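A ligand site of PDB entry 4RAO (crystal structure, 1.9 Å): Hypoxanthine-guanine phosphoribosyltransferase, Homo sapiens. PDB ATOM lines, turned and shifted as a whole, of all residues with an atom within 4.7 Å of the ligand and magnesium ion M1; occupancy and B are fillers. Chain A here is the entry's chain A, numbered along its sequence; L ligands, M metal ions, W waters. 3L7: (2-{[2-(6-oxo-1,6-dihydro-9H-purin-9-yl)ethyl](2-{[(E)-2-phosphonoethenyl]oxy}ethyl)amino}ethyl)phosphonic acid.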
ATOM      1  N   LEU A  67     -12.313  10.869 -10.392  1.00  0.00           N
ATOM      2  CA  LEU A  67     -12.177  12.000 -11.310  1.00  0.00           C
ATOM      3  C   LEU A  67     -13.021  13.178 -10.844  1.00  0.00           C
ATOM      4  O   LEU A  67     -14.001  12.957 -10.132  1.00  0.00           O
ATOM      5  CB  LEU A  67     -12.635  11.557 -12.706  1.00  0.00           C
ATOM      6  CG  LEU A  67     -11.755  10.487 -13.323  1.00  0.00           C
ATOM      7  CD1 LEU A  67     -12.343   9.951 -14.627  1.00  0.00           C
ATOM      8  CD2 LEU A  67     -10.347  11.009 -13.520  1.00  0.00           C
ATOM      9  N   LYS A  68     -12.673  14.402 -11.227  1.00  0.00           N
ATOM     10  CA  LYS A  68     -11.487  14.695 -12.045  1.00  0.00           C
ATOM     11  C   LYS A  68     -10.278  14.968 -11.173  1.00  0.00           C
ATOM     12  O   LYS A  68      -9.139  14.671 -11.563  1.00  0.00           O
ATOM     13  CB  LYS A  68     -11.732  15.941 -12.905  1.00  0.00           C
ATOM     14  CG  LYS A  68     -12.742  15.798 -14.039  1.00  0.00           C
ATOM     15  CD  LYS A  68     -12.925  17.180 -14.665  1.00  0.00           C
ATOM     16  CE  LYS A  68     -13.972  17.228 -15.739  1.00  0.00           C
ATOM     17  NZ  LYS A  68     -13.866  18.562 -16.396  1.00  0.00           N
ATOM     18  N   GLY A  69     -10.526  15.535 -10.002  1.00  0.00           N
ATOM     19  CA  GLY A  69      -9.481  16.077  -9.139  1.00  0.00           C
ATOM     20  C   GLY A  69      -8.503  15.033  -8.626  1.00  0.00           C
ATOM     21  O   GLY A  69      -7.364  15.357  -8.283  1.00  0.00           O
ATOM     22  N   GLY A  70      -8.929  13.788  -8.580  1.00  0.00           N
ATOM     23  CA  GLY A  70      -8.019  12.752  -8.104  1.00  0.00           C
ATOM     24  C   GLY A  70      -6.964  12.285  -9.107  1.00  0.00           C
ATOM     25  O   GLY A  70      -6.081  11.493  -8.739  1.00  0.00           O
ATOM     26  N   ARG A 100     -16.630   8.932 -11.546  1.00  0.00           N
ATOM     27  CA  ARG A 100     -16.831  10.351 -11.338  1.00  0.00           C
ATOM     28  C   ARG A 100     -18.162  10.573 -10.627  1.00  0.00           C
ATOM     29  O   ARG A 100     -19.160   9.940 -10.962  1.00  0.00           O
ATOM     30  CB  ARG A 100     -16.817  11.099 -12.673  1.00  0.00           C
ATOM     31  CG  ARG A 100     -17.305  12.532 -12.554  1.00  0.00           C
ATOM     32  CD  ARG A 100     -16.335  13.508 -13.143  1.00  0.00           C
ATOM     33  NE  ARG A 100     -16.609  13.775 -14.550  1.00  0.00           N
ATOM     34  CZ  ARG A 100     -17.006  14.963 -15.012  1.00  0.00           C
ATOM     35  NH1 ARG A 100     -17.157  15.982 -14.196  1.00  0.00           N
ATOM     36  NH2 ARG A 100     -17.235  15.120 -16.314  1.00  0.00           N
ATOM     37  N   LEU A 101     -18.127  11.453  -9.618  1.00  0.00           N
ATOM     38  CA  LEU A 101     -19.308  11.849  -8.868  1.00  0.00           C
ATOM     39  C   LEU A 101     -19.556  13.349  -9.072  1.00  0.00           C
ATOM     40  O   LEU A 101     -18.603  14.134  -9.085  1.00  0.00           O
ATOM     41  CB  LEU A 101     -19.112  11.567  -7.373  1.00  0.00           C
ATOM     42  CG  LEU A 101     -19.556  10.228  -6.783  1.00  0.00           C
ATOM     43  CD1 LEU A 101     -18.960   9.053  -7.531  1.00  0.00           C
ATOM     44  CD2 LEU A 101     -19.207  10.157  -5.305  1.00  0.00           C
ATOM     45  N   ASP A 134      -8.789  13.294  -4.129  1.00  0.00           N
ATOM     46  CA  ASP A 134      -7.982  14.486  -3.973  1.00  0.00           C
ATOM     47  C   ASP A 134      -8.162  15.129  -2.575  1.00  0.00           C
ATOM     48  O   ASP A 134      -7.174  15.474  -1.905  1.00  0.00           O
ATOM     49  CB  ASP A 134      -8.276  15.521  -5.078  1.00  0.00           C
ATOM     50  CG  ASP A 134      -9.762  15.862  -5.205  1.00  0.00           C
ATOM     51  OD1 ASP A 134     -10.636  15.140  -4.668  1.00  0.00           O
ATOM     52  OD2 ASP A 134     -10.063  16.885  -5.873  1.00  0.00           O
ATOM     53  N   ILE A 135      -9.413  15.288  -2.153  1.00  0.00           N
ATOM     54  CA  ILE A 135      -9.662  15.979  -0.889  1.00  0.00           C
ATOM     55  C   ILE A 135     -10.929  15.471  -0.191  1.00  0.00           C
ATOM     56  O   ILE A 135     -11.946  15.170  -0.828  1.00  0.00           O
ATOM     57  CB  ILE A 135      -9.684  17.522  -1.098  1.00  0.00           C
ATOM     58  CG1 ILE A 135      -9.777  18.263   0.251  1.00  0.00           C
ATOM     59  CG2 ILE A 135     -10.798  17.917  -2.049  1.00  0.00           C
ATOM     60  CD1 ILE A 135      -9.468  19.767   0.176  1.00  0.00           C
ATOM     61  N   ILE A 136     -10.829  15.336   1.122  1.00  0.00           N
ATOM     62  CA  ILE A 136     -11.988  15.075   1.948  1.00  0.00           C
ATOM     63  C   ILE A 136     -12.260  16.315   2.774  1.00  0.00           C
ATOM     64  O   ILE A 136     -11.352  16.864   3.413  1.00  0.00           O
ATOM     65  CB  ILE A 136     -11.780  13.852   2.837  1.00  0.00           C
ATOM     66  CG1 ILE A 136     -11.715  12.601   1.948  1.00  0.00           C
ATOM     67  CG2 ILE A 136     -12.913  13.716   3.870  1.00  0.00           C
ATOM     68  CD1 ILE A 136     -11.373  11.349   2.686  1.00  0.00           C
ATOM     69  N   ASP A 137     -13.496  16.798   2.723  1.00  0.00           N
ATOM     70  CA  ASP A 137     -13.868  17.982   3.474  1.00  0.00           C
ATOM     71  C   ASP A 137     -14.979  17.615   4.457  1.00  0.00           C
ATOM     72  O   ASP A 137     -14.713  17.389   5.629  1.00  0.00           O
ATOM     73  CB  ASP A 137     -14.286  19.124   2.524  1.00  0.00           C
ATOM     74  CG  ASP A 137     -14.734  20.382   3.255  1.00  0.00           C
ATOM     75  OD1 ASP A 137     -14.416  20.547   4.458  1.00  0.00           O
ATOM     76  OD2 ASP A 137     -15.378  21.216   2.602  1.00  0.00           O
ATOM     77  N   THR A 138     -16.220  17.523   3.983  1.00  0.00           N
ATOM     78  CA  THR A 138     -17.310  17.158   4.878  1.00  0.00           C
ATOM     79  C   THR A 138     -17.300  15.645   5.079  1.00  0.00           C
ATOM     80  O   THR A 138     -17.654  15.145   6.139  1.00  0.00           O
ATOM     81  CB  THR A 138     -18.688  17.592   4.335  1.00  0.00           C
ATOM     82  OG1 THR A 138     -18.943  16.930   3.081  1.00  0.00           O
ATOM     83  CG2 THR A 138     -18.748  19.101   4.154  1.00  0.00           C
ATOM     84  N   GLY A 139     -16.869  14.934   4.050  1.00  0.00           N
ATOM     85  CA  GLY A 139     -16.844  13.481   4.088  1.00  0.00           C
ATOM     86  C   GLY A 139     -18.048  12.892   3.366  1.00  0.00           C
ATOM     87  O   GLY A 139     -18.120  11.676   3.180  1.00  0.00           O
ATOM     88  N   LYS A 140     -18.996  13.749   2.979  1.00  0.00           N
ATOM     89  CA  LYS A 140     -20.221  13.269   2.313  1.00  0.00           C
ATOM     90  C   LYS A 140     -19.962  12.489   1.038  1.00  0.00           C
ATOM     91  O   LYS A 140     -20.544  11.428   0.816  1.00  0.00           O
ATOM     92  CB  LYS A 140     -21.150  14.443   1.954  1.00  0.00           C
ATOM     93  CG  LYS A 140     -21.928  15.040   3.102  1.00  0.00           C
ATOM     94  CD  LYS A 140     -23.043  15.936   2.559  1.00  0.00           C
ATOM     95  CE  LYS A 140     -23.610  16.871   3.611  1.00  0.00           C
ATOM     96  NZ  LYS A 140     -22.691  18.023   3.904  1.00  0.00           N
ATOM     97  N   THR A 141     -19.094  13.030   0.187  1.00  0.00           N
ATOM     98  CA  THR A 141     -18.766  12.391  -1.075  1.00  0.00           C
ATOM     99  C   THR A 141     -18.204  10.987  -0.865  1.00  0.00           C
ATOM    100  O   THR A 141     -18.616  10.028  -1.525  1.00  0.00           O
ATOM    101  CB  THR A 141     -17.747  13.210  -1.867  1.00  0.00           C
ATOM    102  OG1 THR A 141     -18.254  14.525  -2.096  1.00  0.00           O
ATOM    103  CG2 THR A 141     -17.450  12.532  -3.206  1.00  0.00           C
ATOM    104  N   MET A 142     -17.266  10.869   0.060  1.00  0.00           N
ATOM    105  CA  MET A 142     -16.641   9.566   0.303  1.00  0.00           C
ATOM    106  C   MET A 142     -17.626   8.549   0.886  1.00  0.00           C
ATOM    107  O   MET A 142     -17.671   7.396   0.436  1.00  0.00           O
ATOM    108  CB  MET A 142     -15.392   9.720   1.196  1.00  0.00           C
ATOM    109  CG  MET A 142     -14.490   8.495   1.143  1.00  0.00           C
ATOM    110  SD  MET A 142     -14.336   7.758  -0.507  1.00  0.00           S
ATOM    111  CE  MET A 142     -13.555   9.090  -1.425  1.00  0.00           C
ATOM    112  N   LYS A 165      -9.345  18.112   5.065  1.00  0.00           N
ATOM    113  CA  LYS A 165      -9.546  19.414   5.685  1.00  0.00           C
ATOM    114  C   LYS A 165      -9.957  19.257   7.129  1.00  0.00           C
ATOM    115  O   LYS A 165     -10.806  18.415   7.455  1.00  0.00           O
ATOM    116  CB  LYS A 165     -10.629  20.200   4.952  1.00  0.00           C
ATOM    117  CG  LYS A 165     -10.167  20.884   3.677  1.00  0.00           C
ATOM    118  CD  LYS A 165     -10.934  22.192   3.482  1.00  0.00           C
ATOM    119  CE  LYS A 165     -10.546  22.796   2.155  1.00  0.00           C
ATOM    120  NZ  LYS A 165     -11.489  23.814   1.660  1.00  0.00           N
ATOM    121  N   LYS A 185      -9.120  26.237   4.322  1.00  0.00           N
ATOM    122  CA  LYS A 185      -8.815  27.261   3.321  1.00  0.00           C
ATOM    123  C   LYS A 185      -9.081  26.628   1.978  1.00  0.00           C
ATOM    124  O   LYS A 185      -8.909  25.421   1.834  1.00  0.00           O
ATOM    125  CB  LYS A 185      -7.320  27.613   3.350  1.00  0.00           C
ATOM    126  CG  LYS A 185      -6.829  28.342   4.572  1.00  0.00           C
ATOM    127  CD  LYS A 185      -5.311  28.486   4.496  1.00  0.00           C
ATOM    128  CE  LYS A 185      -4.864  29.929   4.663  1.00  0.00           C
ATOM    129  NZ  LYS A 185      -5.293  30.466   5.975  1.00  0.00           N
ATOM    130  N   PHE A 186      -9.473  27.409   0.989  1.00  0.00           N
ATOM    131  CA  PHE A 186      -9.692  26.834  -0.345  1.00  0.00           C
ATOM    132  C   PHE A 186      -8.378  26.704  -1.103  1.00  0.00           C
ATOM    133  O   PHE A 186      -7.646  27.695  -1.261  1.00  0.00           O
ATOM    134  CB  PHE A 186     -10.685  27.663  -1.156  1.00  0.00           C
ATOM    135  CG  PHE A 186     -11.261  26.931  -2.321  1.00  0.00           C
ATOM    136  CD1 PHE A 186     -10.639  26.982  -3.565  1.00  0.00           C
ATOM    137  CD2 PHE A 186     -12.419  26.176  -2.182  1.00  0.00           C
ATOM    138  CE1 PHE A 186     -11.169  26.286  -4.649  1.00  0.00           C
ATOM    139  CE2 PHE A 186     -12.953  25.476  -3.253  1.00  0.00           C
ATOM    140  CZ  PHE A 186     -12.326  25.533  -4.493  1.00  0.00           C
ATOM    141  N   VAL A 187      -8.064  25.487  -1.557  1.00  0.00           N
ATOM    142  CA  VAL A 187      -6.818  25.251  -2.255  1.00  0.00           C
ATOM    143  C   VAL A 187      -7.059  24.715  -3.661  1.00  0.00           C
ATOM    144  O   VAL A 187      -8.091  24.088  -3.925  1.00  0.00           O
ATOM    145  CB  VAL A 187      -5.883  24.283  -1.492  1.00  0.00           C
ATOM    146  CG1 VAL A 187      -5.456  24.889  -0.167  1.00  0.00           C
ATOM    147  CG2 VAL A 187      -6.562  22.941  -1.293  1.00  0.00           C
ATOM    148  N   LEU A 192      -6.574  19.759  -8.483  1.00  0.00           N
ATOM    149  CA  LEU A 192      -7.694  20.366  -7.768  1.00  0.00           C
ATOM    150  C   LEU A 192      -8.119  21.673  -8.448  1.00  0.00           C
ATOM    151  O   LEU A 192      -7.283  22.509  -8.772  1.00  0.00           O
ATOM    152  CB  LEU A 192      -7.364  20.607  -6.294  1.00  0.00           C
ATOM    153  CG  LEU A 192      -7.382  19.363  -5.389  1.00  0.00           C
ATOM    154  CD1 LEU A 192      -6.088  18.577  -5.471  1.00  0.00           C
ATOM    155  CD2 LEU A 192      -7.657  19.768  -3.940  1.00  0.00           C
ATOM    156  N   ASP A 193      -9.417  21.864  -8.637  1.00  0.00           N
ATOM    157  CA  ASP A 193      -9.857  23.005  -9.417  1.00  0.00           C
ATOM    158  C   ASP A 193     -10.633  24.059  -8.648  1.00  0.00           C
ATOM    159  O   ASP A 193     -11.143  23.818  -7.550  1.00  0.00           O
ATOM    160  CB  ASP A 193     -10.746  22.539 -10.564  1.00  0.00           C
ATOM    161  CG  ASP A 193     -12.130  22.163 -10.086  1.00  0.00           C
ATOM    162  OD1 ASP A 193     -12.237  21.361  -9.147  1.00  0.00           O
ATOM    163  OD2 ASP A 193     -13.108  22.698 -10.645  1.00  0.00           O
ATOM    164  N   ARG A 199      -6.312  23.207 -12.618  1.00  0.00           N
ATOM    165  CA  ARG A 199      -5.910  21.792 -12.623  1.00  0.00           C
ATOM    166  C   ARG A 199      -4.523  21.608 -13.224  1.00  0.00           C
ATOM    167  O   ARG A 199      -3.763  20.711 -12.816  1.00  0.00           O
ATOM    168  CB  ARG A 199      -6.936  20.928 -13.365  1.00  0.00           C
ATOM    169  CG  ARG A 199      -8.346  20.938 -12.741  1.00  0.00           C
ATOM    170  CD  ARG A 199      -9.168  19.723 -13.219  1.00  0.00           C
ATOM    171  NE  ARG A 199     -10.603  19.842 -12.987  1.00  0.00           N
ATOM    172  CZ  ARG A 199     -11.248  19.457 -11.884  1.00  0.00           C
ATOM    173  NH1 ARG A 199     -10.581  18.938 -10.855  1.00  0.00           N
ATOM    174  NH2 ARG A 199     -12.571  19.621 -11.802  1.00  0.00           N
HETATM  175  OAD 3L7 L   1     -13.924  18.732  -9.380  1.00  0.00           O
HETATM  176  PBA 3L7 L   1     -14.089  17.146  -9.313  1.00  0.00           P
HETATM  177  OAE 3L7 L   1     -12.712  16.490  -9.115  1.00  0.00           O
HETATM  178  OAB 3L7 L   1     -14.714  16.633 -10.587  1.00  0.00           O
HETATM  179  CAP 3L7 L   1     -15.152  16.655  -7.839  1.00  0.00           C
HETATM  180  CAK 3L7 L   1     -16.085  17.671  -7.190  1.00  0.00           C
HETATM  181  OAU 3L7 L   1     -17.057  17.181  -6.355  1.00  0.00           O
HETATM  182  CAJ 3L7 L   1     -16.767  16.943  -5.050  1.00  0.00           C
HETATM  183  CAL 3L7 L   1     -16.294  18.126  -4.216  1.00  0.00           C
HETATM  184  NAY 3L7 L   1     -15.450  17.795  -3.052  1.00  0.00           N
HETATM  185  CAN 3L7 L   1     -16.242  17.669  -1.819  1.00  0.00           C
HETATM  186  CAQ 3L7 L   1     -15.734  16.638  -0.838  1.00  0.00           C
HETATM  187  PBB 3L7 L   1     -16.680  16.382   0.648  1.00  0.00           P
HETATM  188  OAF 3L7 L   1     -17.154  17.717   1.240  1.00  0.00           O
HETATM  189  OAG 3L7 L   1     -17.930  15.471   0.307  1.00  0.00           O
HETATM  190  OAC 3L7 L   1     -15.861  15.656   1.635  1.00  0.00           O
HETATM  191  CAM 3L7 L   1     -14.414  18.831  -2.872  1.00  0.00           C
HETATM  192  CAO 3L7 L   1     -14.868  20.230  -2.682  1.00  0.00           C
HETATM  193  N9  3L7 L   1     -13.842  21.038  -1.923  1.00  0.00           N
HETATM  194  C4  3L7 L   1     -12.712  21.615  -2.503  1.00  0.00           C
HETATM  195  N3  3L7 L   1     -12.236  21.664  -3.849  1.00  0.00           N
HETATM  196  C2  3L7 L   1     -11.086  22.328  -4.118  1.00  0.00           C
HETATM  197  N1  3L7 L   1     -10.390  22.946  -3.113  1.00  0.00           N
HETATM  198  C6  3L7 L   1     -10.795  22.940  -1.805  1.00  0.00           C
HETATM  199  O6  3L7 L   1     -10.085  23.564  -0.865  1.00  0.00           O
HETATM  200  C5  3L7 L   1     -12.018  22.242  -1.487  1.00  0.00           C
HETATM  201  N7  3L7 L   1     -12.732  22.021  -0.291  1.00  0.00           N
HETATM  202  C8  3L7 L   1     -13.822  21.276  -0.593  1.00  0.00           C
HETATM  203 MG    MG M   1     -14.306  20.874  -8.339  1.00  0.00          MG
HETATM  204 MG    MG M   2     -12.829  14.499  -5.215  1.00  0.00          MG
HETATM  205  O   HOH W   1     -13.724  23.021  -6.967  1.00  0.00           O
HETATM  206  O   HOH W   2     -12.335  14.050  -7.405  1.00  0.00           O
HETATM  207  O   HOH W   3     -10.920  18.969  -7.428  1.00  0.00           O
HETATM  208  O   HOH W   4     -13.403  15.813  -3.268  1.00  0.00           O
HETATM  209  O   HOH W   5     -15.624  13.038   1.011  1.00  0.00           O
HETATM  210  O   HOH W   6     -14.927  14.045  -5.761  1.00  0.00           O
HETATM  211  O   HOH W   7     -12.799  16.579  -6.156  1.00  0.00           O
HETATM  212  O   HOH W   8     -13.015  19.932  -6.118  1.00  0.00           O
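An oxygen (OAE) of the ligand lies within hydrogen-bond range of the backbone NH (N) of Gly 69 (2.5 Å). N of Thr 141 sits at hydrogen-bond distance from OAG of the ligand (2.7 Å). OG1 of Thr 141 sits at hydrogen-bond distance from OAG of the ligand (2.6 Å). The backbone NH (N) of Thr 138 sits at hydrogen-bond distance from an oxygen (OAF) of the ligand (2.9 Å). OG1 of Thr 138 sits at hydrogen-bond distance from OAF of the ligand. An oxygen (O6) of the ligand lies within hydrogen-bond range of the backbone NH (N) of Val 187, at 2.9 Å. O of Val 187 is in hydrogen-bond range of N1 of the ligand, at 2.7 Å. The backbone NH (N) of Gly 139 is in hydrogen-bond range of an oxygen (OAC) of the ligand (2.7 Å). The backbone NH (N) of Asp 137 sits at hydrogen-bond distance from an oxygen (OAC) of the ligand, 2.8 Å away. The side-chain amino group (NZ) of Lys 165 lies within hydrogen-bond range of an oxygen (O6) of the ligand, at 2.9 Å. OAE of the ligand is in salt-bridge range of NH1 of Arg 199, 3.7 Å away. OAE of the ligand is in hydrogen-bond range of N of Lys 68, 3.0 Å away. An oxygen (OAG) of the ligand lies within hydrogen-bond range of the backbone NH (N) of Lys 140 (3.4 Å).
The guanidinium group (NH2) of Arg 199 lies within salt-bridge range of the side-chain carboxylate (OD2) of Asp 193 (3.3 Å). The side-chain hydroxyl of Thr 138 lies within hydrogen-bond range of the backbone NH of Lys 140 (3.2 Å). NZ of Lys 165 is in hydrogen-bond range of O of Lys 185 (3.0 Å). N of Lys 165 lies within hydrogen-bond range of O of Ile 136 (2.9 Å).
The backbone carbonyl oxygen (O) of Lys 185 sits close to an oxygen (O6) of the ligand (3.5 Å). Leu 67 touches the ligand (C to OAE, 3.7 Å). Ile 135 touches the ligand (CG2 to CAM, 3.8 Å). Ile 136 touches the ligand (C to OAC, 3.8 Å). Phe 186 touches the ligand (CA to O6, 3.3 Å). 16 residues have an atom within 4 Å of the ligand: Leu 67, Lys 68, Gly 69, Ile 135, Ile 136, Asp 137, Thr 138, Gly 139, Lys 140, Thr 141, Lys 165, Lys 185, Phe 186, Val 187, Asp 193 and Arg 199. The nearest printed residue that does not touch the ligand is Asp 134 (4.2 Å).
One residue has an atom within 4 Å of magnesium ion M1: Asp 193. The nearest printed residue that does not touch magnesium ion M1 is Arg 199 (4.1 Å).
Magnesium ion M1 is bound by the side-chain carboxylate of Asp 193 (2.3 Å) and an oxygen (OAD) of the ligand (2.4 Å). Slightly farther from magnesium ion M1 lies water W1 (2.6 Å). Slightly farther from magnesium ion M1 lies water W8 (2.7 Å).
Water W5 lies within hydrogen-bond range of OAC of the ligand and N of Met 142. Water W7 bridges the side-chain carboxylate of Asp 134 and an oxygen (OAE) of the ligand. Water W2 lies within hydrogen-bond range of an oxygen (OAE) of the ligand, the backbone carbonyl oxygen of Leu 67 and the backbone NH of Gly 69. Water W3 lies within hydrogen-bond range of OD2 of Asp 134 (2.7 Å), NH1 of Arg 199 (3.4 Å), N of Asp 193 (3.5 Å) and OAE of the ligand (3.5 Å).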
